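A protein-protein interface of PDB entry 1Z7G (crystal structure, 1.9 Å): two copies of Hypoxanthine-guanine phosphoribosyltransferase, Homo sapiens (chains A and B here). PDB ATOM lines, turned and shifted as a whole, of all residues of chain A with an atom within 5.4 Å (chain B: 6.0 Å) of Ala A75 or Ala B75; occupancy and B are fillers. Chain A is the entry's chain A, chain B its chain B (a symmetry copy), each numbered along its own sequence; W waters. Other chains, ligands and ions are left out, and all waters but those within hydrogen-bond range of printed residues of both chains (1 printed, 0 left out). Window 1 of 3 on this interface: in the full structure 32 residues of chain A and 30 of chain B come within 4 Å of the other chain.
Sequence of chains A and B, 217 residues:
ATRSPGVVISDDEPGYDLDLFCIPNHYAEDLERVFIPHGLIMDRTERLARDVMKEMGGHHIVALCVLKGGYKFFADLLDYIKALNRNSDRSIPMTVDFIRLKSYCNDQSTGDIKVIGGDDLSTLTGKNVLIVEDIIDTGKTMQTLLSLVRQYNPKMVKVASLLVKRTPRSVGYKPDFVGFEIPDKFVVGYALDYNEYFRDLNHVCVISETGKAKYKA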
ATOM      1  N   TYR A  71     -31.895 -16.987   7.127  1.00  0.00           N
ATOM      2  CA  TYR A  71     -32.199 -15.617   7.550  1.00  0.00           C
ATOM      3  C   TYR A  71     -31.546 -14.622   6.593  1.00  0.00           C
ATOM      4  O   TYR A  71     -31.950 -13.458   6.501  1.00  0.00           O
ATOM      5  CB  TYR A  71     -31.656 -15.372   8.965  1.00  0.00           C
ATOM      6  CG  TYR A  71     -30.142 -15.323   9.022  1.00  0.00           C
ATOM      7  CD1 TYR A  71     -29.449 -14.149   8.718  1.00  0.00           C
ATOM      8  CD2 TYR A  71     -29.398 -16.471   9.313  1.00  0.00           C
ATOM      9  CE1 TYR A  71     -28.047 -14.116   8.700  1.00  0.00           C
ATOM     10  CE2 TYR A  71     -28.001 -16.453   9.296  1.00  0.00           C
ATOM     11  CZ  TYR A  71     -27.330 -15.272   8.985  1.00  0.00           C
ATOM     12  OH  TYR A  71     -25.951 -15.258   8.935  1.00  0.00           O
ATOM     13  N   LYS A  72     -30.526 -15.101   5.891  1.00  0.00           N
ATOM     14  CA  LYS A  72     -29.769 -14.283   4.963  1.00  0.00           C
ATOM     15  C   LYS A  72     -30.604 -13.430   4.031  1.00  0.00           C
ATOM     16  O   LYS A  72     -30.440 -12.217   4.007  1.00  0.00           O
ATOM     17  CB  LYS A  72     -28.835 -15.155   4.128  1.00  0.00           C
ATOM     18  CG  LYS A  72     -27.353 -14.932   4.380  1.00  0.00           C
ATOM     19  CD  LYS A  72     -26.946 -13.482   4.155  1.00  0.00           C
ATOM     20  CE  LYS A  72     -26.820 -12.729   5.471  1.00  0.00           C
ATOM     21  NZ  LYS A  72     -26.403 -11.306   5.287  1.00  0.00           N
ATOM     22  N   PHE A  73     -31.489 -14.043   3.253  1.00  0.00           N
ATOM     23  CA  PHE A  73     -32.276 -13.241   2.326  1.00  0.00           C
ATOM     24  C   PHE A  73     -33.093 -12.168   3.046  1.00  0.00           C
ATOM     25  O   PHE A  73     -33.146 -11.023   2.600  1.00  0.00           O
ATOM     26  CB  PHE A  73     -33.199 -14.104   1.466  1.00  0.00           C
ATOM     27  CG  PHE A  73     -33.974 -13.309   0.447  1.00  0.00           C
ATOM     28  CD1 PHE A  73     -33.308 -12.496  -0.467  1.00  0.00           C
ATOM     29  CD2 PHE A  73     -35.369 -13.334   0.432  1.00  0.00           C
ATOM     30  CE1 PHE A  73     -34.020 -11.712  -1.384  1.00  0.00           C
ATOM     31  CE2 PHE A  73     -36.090 -12.562  -0.471  1.00  0.00           C
ATOM     32  CZ  PHE A  73     -35.418 -11.745  -1.384  1.00  0.00           C
ATOM     33  N   PHE A  74     -33.727 -12.537   4.154  1.00  0.00           N
ATOM     34  CA  PHE A  74     -34.524 -11.577   4.913  1.00  0.00           C
ATOM     35  C   PHE A  74     -33.652 -10.402   5.319  1.00  0.00           C
ATOM     36  O   PHE A  74     -34.020  -9.240   5.134  1.00  0.00           O
ATOM     37  CB  PHE A  74     -35.090 -12.243   6.169  1.00  0.00           C
ATOM     38  CG  PHE A  74     -35.969 -13.418   5.878  1.00  0.00           C
ATOM     39  CD1 PHE A  74     -36.081 -14.464   6.786  1.00  0.00           C
ATOM     40  CD2 PHE A  74     -36.687 -13.482   4.687  1.00  0.00           C
ATOM     41  CE1 PHE A  74     -36.902 -15.564   6.503  1.00  0.00           C
ATOM     42  CE2 PHE A  74     -37.503 -14.571   4.399  1.00  0.00           C
ATOM     43  CZ  PHE A  74     -37.612 -15.611   5.305  1.00  0.00           C
ATOM     44  N   ALA A  75     -32.492 -10.722   5.879  1.00  0.00           N
ATOM     45  CA  ALA A  75     -31.548  -9.715   6.341  1.00  0.00           C
ATOM     46  C   ALA A  75     -31.053  -8.780   5.243  1.00  0.00           C
ATOM     47  O   ALA A  75     -31.053  -7.562   5.416  1.00  0.00           O
ATOM     48  CB  ALA A  75     -30.359 -10.392   7.020  1.00  0.00           C
ATOM     49  N   ASP A  76     -30.620  -9.341   4.120  1.00  0.00           N
ATOM     50  CA  ASP A  76     -30.119  -8.515   3.032  1.00  0.00           C
ATOM     51  C   ASP A  76     -31.219  -7.659   2.420  1.00  0.00           C
ATOM     52  O   ASP A  76     -31.024  -6.468   2.198  1.00  0.00           O
ATOM     53  CB  ASP A  76     -29.452  -9.397   1.968  1.00  0.00           C
ATOM     54  CG  ASP A  76     -28.115  -9.967   2.435  1.00  0.00           C
ATOM     55  OD1 ASP A  76     -27.622 -10.933   1.815  1.00  0.00           O
ATOM     56  OD2 ASP A  76     -27.549  -9.442   3.422  1.00  0.00           O
ATOM     57  N   LEU A  77     -32.382  -8.243   2.160  1.00  0.00           N
ATOM     58  CA  LEU A  77     -33.481  -7.461   1.590  1.00  0.00           C
ATOM     59  C   LEU A  77     -33.832  -6.317   2.544  1.00  0.00           C
ATOM     60  O   LEU A  77     -33.931  -5.161   2.130  1.00  0.00           O
ATOM     61  CB  LEU A  77     -34.720  -8.337   1.364  1.00  0.00           C
ATOM     62  CG  LEU A  77     -35.963  -7.652   0.768  1.00  0.00           C
ATOM     63  CD1 LEU A  77     -35.662  -7.114  -0.632  1.00  0.00           C
ATOM     64  CD2 LEU A  77     -37.115  -8.648   0.715  1.00  0.00           C
ATOM     65  N   LEU A  78     -34.006  -6.641   3.821  1.00  0.00           N
ATOM     66  CA  LEU A  78     -34.342  -5.617   4.810  1.00  0.00           C
ATOM     67  C   LEU A  78     -33.249  -4.557   4.951  1.00  0.00           C
ATOM     68  O   LEU A  78     -33.556  -3.376   5.133  1.00  0.00           O
ATOM     69  CB  LEU A  78     -34.640  -6.263   6.164  1.00  0.00           C
ATOM     70  CG  LEU A  78     -35.937  -7.077   6.145  1.00  0.00           C
ATOM     71  CD1 LEU A  78     -36.105  -7.832   7.441  1.00  0.00           C
ATOM     72  CD2 LEU A  78     -37.110  -6.142   5.900  1.00  0.00           C
ATOM     73  N   ASP A  79     -31.982  -4.967   4.858  1.00  0.00           N
ATOM     74  CA  ASP A  79     -30.875  -4.010   4.958  1.00  0.00           C
ATOM     75  C   ASP A  79     -30.946  -2.990   3.823  1.00  0.00           C
ATOM     76  O   ASP A  79     -30.774  -1.796   4.046  1.00  0.00           O
ATOM     77  CB  ASP A  79     -29.514  -4.709   4.899  1.00  0.00           C
ATOM     78  CG  ASP A  79     -29.161  -5.439   6.185  1.00  0.00           C
ATOM     79  OD1 ASP A  79     -29.844  -5.247   7.220  1.00  0.00           O
ATOM     80  OD2 ASP A  79     -28.179  -6.207   6.156  1.00  0.00           O
ATOM     81  N   TYR A  80     -31.193  -3.460   2.600  1.00  0.00           N
ATOM     82  CA  TYR A  80     -31.292  -2.558   1.458  1.00  0.00           C
ATOM     83  C   TYR A  80     -32.527  -1.667   1.566  1.00  0.00           C
ATOM     84  O   TYR A  80     -32.491  -0.502   1.169  1.00  0.00           O
ATOM     85  CB  TYR A  80     -31.341  -3.348   0.139  1.00  0.00           C
ATOM     86  CG  TYR A  80     -29.988  -3.846  -0.347  1.00  0.00           C
ATOM     87  CD1 TYR A  80     -29.715  -5.211  -0.449  1.00  0.00           C
ATOM     88  CD2 TYR A  80     -28.984  -2.943  -0.710  1.00  0.00           C
ATOM     89  CE1 TYR A  80     -28.473  -5.670  -0.901  1.00  0.00           C
ATOM     90  CE2 TYR A  80     -27.736  -3.390  -1.163  1.00  0.00           C
ATOM     91  CZ  TYR A  80     -27.488  -4.754  -1.253  1.00  0.00           C
ATOM     92  OH  TYR A  80     -26.252  -5.193  -1.679  1.00  0.00           O
ATOM     93  N   TYR B  71     -33.205  -7.853  14.047  1.00  0.00           N
ATOM     94  CA  TYR B  71     -32.549  -9.019  13.457  1.00  0.00           C
ATOM     95  C   TYR B  71     -31.068  -8.763  13.162  1.00  0.00           C
ATOM     96  O   TYR B  71     -30.299  -9.707  12.986  1.00  0.00           O
ATOM     97  CB  TYR B  71     -33.253  -9.415  12.153  1.00  0.00           C
ATOM     98  CG  TYR B  71     -33.003  -8.437  11.026  1.00  0.00           C
ATOM     99  CD1 TYR B  71     -31.825  -8.490  10.271  1.00  0.00           C
ATOM    100  CD2 TYR B  71     -33.903  -7.404  10.771  1.00  0.00           C
ATOM    101  CE1 TYR B  71     -31.546  -7.529   9.293  1.00  0.00           C
ATOM    102  CE2 TYR B  71     -33.637  -6.437   9.797  1.00  0.00           C
ATOM    103  CZ  TYR B  71     -32.455  -6.502   9.065  1.00  0.00           C
ATOM    104  OH  TYR B  71     -32.174  -5.521   8.139  1.00  0.00           O
ATOM    105  N   LYS B  72     -30.676  -7.491  13.106  1.00  0.00           N
ATOM    106  CA  LYS B  72     -29.293  -7.119  12.790  1.00  0.00           C
ATOM    107  C   LYS B  72     -28.203  -7.833  13.574  1.00  0.00           C
ATOM    108  O   LYS B  72     -27.266  -8.368  12.977  1.00  0.00           O
ATOM    109  CB  LYS B  72     -29.096  -5.609  12.948  1.00  0.00           C
ATOM    110  CG  LYS B  72     -29.705  -4.763  11.843  1.00  0.00           C
ATOM    111  CD  LYS B  72     -28.684  -4.424  10.764  1.00  0.00           C
ATOM    112  CE  LYS B  72     -28.296  -5.641   9.932  1.00  0.00           C
ATOM    113  NZ  LYS B  72     -27.391  -5.250   8.813  1.00  0.00           N
ATOM    114  N   PHE B  73     -28.302  -7.842  14.900  1.00  0.00           N
ATOM    115  CA  PHE B  73     -27.264  -8.499  15.685  1.00  0.00           C
ATOM    116  C   PHE B  73     -27.156  -9.984  15.353  1.00  0.00           C
ATOM    117  O   PHE B  73     -26.054 -10.500  15.190  1.00  0.00           O
ATOM    118  CB  PHE B  73     -27.493  -8.324  17.184  1.00  0.00           C
ATOM    119  CG  PHE B  73     -26.402  -8.933  18.026  1.00  0.00           C
ATOM    120  CD1 PHE B  73     -25.072  -8.564  17.827  1.00  0.00           C
ATOM    121  CD2 PHE B  73     -26.699  -9.887  19.000  1.00  0.00           C
ATOM    122  CE1 PHE B  73     -24.046  -9.137  18.587  1.00  0.00           C
ATOM    123  CE2 PHE B  73     -25.686 -10.466  19.766  1.00  0.00           C
ATOM    124  CZ  PHE B  73     -24.353 -10.088  19.557  1.00  0.00           C
ATOM    125  N   PHE B  74     -28.294 -10.665  15.251  1.00  0.00           N
ATOM    126  CA  PHE B  74     -28.297 -12.089  14.917  1.00  0.00           C
ATOM    127  C   PHE B  74     -27.610 -12.310  13.571  1.00  0.00           C
ATOM    128  O   PHE B  74     -26.751 -13.177  13.438  1.00  0.00           O
ATOM    129  CB  PHE B  74     -29.732 -12.613  14.837  1.00  0.00           C
ATOM    130  CG  PHE B  74     -30.550 -12.320  16.056  1.00  0.00           C
ATOM    131  CD1 PHE B  74     -31.908 -12.052  15.942  1.00  0.00           C
ATOM    132  CD2 PHE B  74     -29.968 -12.304  17.323  1.00  0.00           C
ATOM    133  CE1 PHE B  74     -32.681 -11.771  17.076  1.00  0.00           C
ATOM    134  CE2 PHE B  74     -30.733 -12.026  18.461  1.00  0.00           C
ATOM    135  CZ  PHE B  74     -32.088 -11.759  18.336  1.00  0.00           C
ATOM    136  N   ALA B  75     -27.997 -11.516  12.579  1.00  0.00           N
ATOM    137  CA  ALA B  75     -27.424 -11.627  11.242  1.00  0.00           C
ATOM    138  C   ALA B  75     -25.921 -11.346  11.198  1.00  0.00           C
ATOM    139  O   ALA B  75     -25.166 -12.087  10.565  1.00  0.00           O
ATOM    140  CB  ALA B  75     -28.160 -10.690  10.287  1.00  0.00           C
ATOM    141  N   ASP B  76     -25.488 -10.285  11.870  1.00  0.00           N
ATOM    142  CA  ASP B  76     -24.077  -9.918  11.888  1.00  0.00           C
ATOM    143  C   ASP B  76     -23.224 -10.944  12.615  1.00  0.00           C
ATOM    144  O   ASP B  76     -22.187 -11.359  12.106  1.00  0.00           O
ATOM    145  CB  ASP B  76     -23.899  -8.528  12.516  1.00  0.00           C
ATOM    146  CG  ASP B  76     -24.347  -7.406  11.585  1.00  0.00           C
ATOM    147  OD1 ASP B  76     -24.648  -6.303  12.079  1.00  0.00           O
ATOM    148  OD2 ASP B  76     -24.394  -7.618  10.356  1.00  0.00           O
ATOM    149  N   LEU B  77     -23.666 -11.368  13.794  1.00  0.00           N
ATOM    150  CA  LEU B  77     -22.925 -12.362  14.561  1.00  0.00           C
ATOM    151  C   LEU B  77     -22.791 -13.648  13.756  1.00  0.00           C
ATOM    152  O   LEU B  77     -21.689 -14.183  13.602  1.00  0.00           O
ATOM    153  CB  LEU B  77     -23.637 -12.670  15.887  1.00  0.00           C
ATOM    154  CG  LEU B  77     -22.967 -13.765  16.728  1.00  0.00           C
ATOM    155  CD1 LEU B  77     -21.550 -13.327  17.088  1.00  0.00           C
ATOM    156  CD2 LEU B  77     -23.783 -14.042  17.983  1.00  0.00           C
ATOM    157  N   LEU B  78     -23.918 -14.135  13.244  1.00  0.00           N
ATOM    158  CA  LEU B  78     -23.938 -15.359  12.447  1.00  0.00           C
ATOM    159  C   LEU B  78     -23.139 -15.221  11.147  1.00  0.00           C
ATOM    160  O   LEU B  78     -22.505 -16.180  10.701  1.00  0.00           O
ATOM    161  CB  LEU B  78     -25.384 -15.772  12.152  1.00  0.00           C
ATOM    162  CG  LEU B  78     -26.221 -16.262  13.344  1.00  0.00           C
ATOM    163  CD1 LEU B  78     -27.645 -16.600  12.884  1.00  0.00           C
ATOM    164  CD2 LEU B  78     -25.563 -17.485  13.979  1.00  0.00           C
ATOM    165  N   ASP B  79     -23.158 -14.039  10.535  1.00  0.00           N
ATOM    166  CA  ASP B  79     -22.387 -13.829   9.305  1.00  0.00           C
ATOM    167  C   ASP B  79     -20.893 -13.971   9.612  1.00  0.00           C
ATOM    168  O   ASP B  79     -20.153 -14.586   8.851  1.00  0.00           O
ATOM    169  CB  ASP B  79     -22.635 -12.436   8.705  1.00  0.00           C
ATOM    170  CG  ASP B  79     -23.956 -12.332   7.937  1.00  0.00           C
ATOM    171  OD1 ASP B  79     -24.622 -13.358   7.694  1.00  0.00           O
ATOM    172  OD2 ASP B  79     -24.327 -11.199   7.563  1.00  0.00           O
ATOM    173  N   TYR B  80     -20.440 -13.396  10.724  1.00  0.00           N
ATOM    174  CA  TYR B  80     -19.022 -13.489  11.077  1.00  0.00           C
ATOM    175  C   TYR B  80     -18.637 -14.912  11.450  1.00  0.00           C
ATOM    176  O   TYR B  80     -17.552 -15.382  11.104  1.00  0.00           O
ATOM    177  CB  TYR B  80     -18.678 -12.542  12.233  1.00  0.00           C
ATOM    178  CG  TYR B  80     -18.494 -11.102  11.812  1.00  0.00           C
ATOM    179  CD1 TYR B  80     -19.383 -10.109  12.237  1.00  0.00           C
ATOM    180  CD2 TYR B  80     -17.413 -10.722  11.014  1.00  0.00           C
ATOM    181  CE1 TYR B  80     -19.193  -8.768  11.880  1.00  0.00           C
ATOM    182  CE2 TYR B  80     -17.213  -9.389  10.649  1.00  0.00           C
ATOM    183  CZ  TYR B  80     -18.108  -8.416  11.089  1.00  0.00           C
ATOM    184  OH  TYR B  80     -17.918  -7.096  10.750  1.00  0.00           O
HETATM  185  O   HOH W   1     -27.297  -7.938   7.851  1.00  0.00           O
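Ala A75 touches just these residues of chain B: Tyr B71 and Ala B75. Printed residues of chain A within 4 Å of Asp B79: Tyr A71 (2.6 Å) and Lys A72 (3.1 Å). Of the printed residues of chain B, Tyr A71 touches Ala B75 (3.6 Å), Leu B78 (3.3 Å) and Asp B79 (2.6 Å). Of the printed residues of chain B, Lys A72 touches Asp B79 (3.1 Å). Of the printed residues of chain A, Tyr B71 touches Ala A75 (3.6 Å), Leu A78 (3.2 Å) and Asp A79 (2.5 Å). Of the printed residues of chain A, Lys B72 touches Asp A79. The nearest residue of chain B that does not touch Ala A75 is Lys B72 (5.5 Å). The nearest printed residue of chain A that does not touch Lys B72 is Ala A75 (5.5 Å).
NZ of Lys A72 lies within salt-bridge range of OD2 of Asp A76 (2.9 Å).
Tyr A71 touches Leu B78, and with the chains exchanged Leu A78 touches Tyr B71. Tyr A71 touches Asp B79, and with the chains exchanged Asp A79 touches Tyr B71. Lys A72 touches Asp B79, and with the chains exchanged Asp A79 touches Lys B72. Ala B75 touches its own counterpart, Ala A75. 10 positions are printed for both chains. Of the 9 pairs that touch across the chains among the printed residues, 9 have their exchanged pair printed and touching as well.
The side-chain carboxylate of Asp B79 lies within salt-bridge range of the side-chain amino group of Lys A72. The side-chain amino group (NZ) of Lys B72 is in salt-bridge range of the side-chain carboxylate (OD1) of Asp A79 (2.9 Å). The side-chain hydroxyl (OH) of Tyr A71 sits at hydrogen-bond distance from the side-chain carboxylate (OD1) of Asp B79 (2.6 Å). The side-chain hydroxyl of Tyr B71 is in hydrogen-bond range of the side-chain carboxylate of Asp A79, 2.5 Å away.
Water W1 lies within hydrogen-bond range of the side-chain carboxylate of Asp A79 and the side-chain amino group of Lys B72.
Hydrophobic or aromatic side chains of chain B within 4 Å of the printed part of chain A: Tyr B71, Ala B75 and Leu B78. Of the 10 printed residues of chain A, 5 touch a printed residue of chain B. Hydrophobic or aromatic side chains of chain A within 4 Å of the printed part of chain B: Tyr A71, Ala A75 and Leu A78. Along chain A the printed residues that touch a printed residue of chain B span positions 71 to 79.
CE1 of Tyr A71 touches CA of Ala B75, 3.6 Å away. Tyr A71 touches Leu B78 (OH to CB, 3.3 Å). Tyr B71 touches Ala A75. Ala A75 touches Ala B75 (CB to CB, 3.9 Å). Leu A78 touches Tyr B71 (CB to OH, 3.2 Å).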
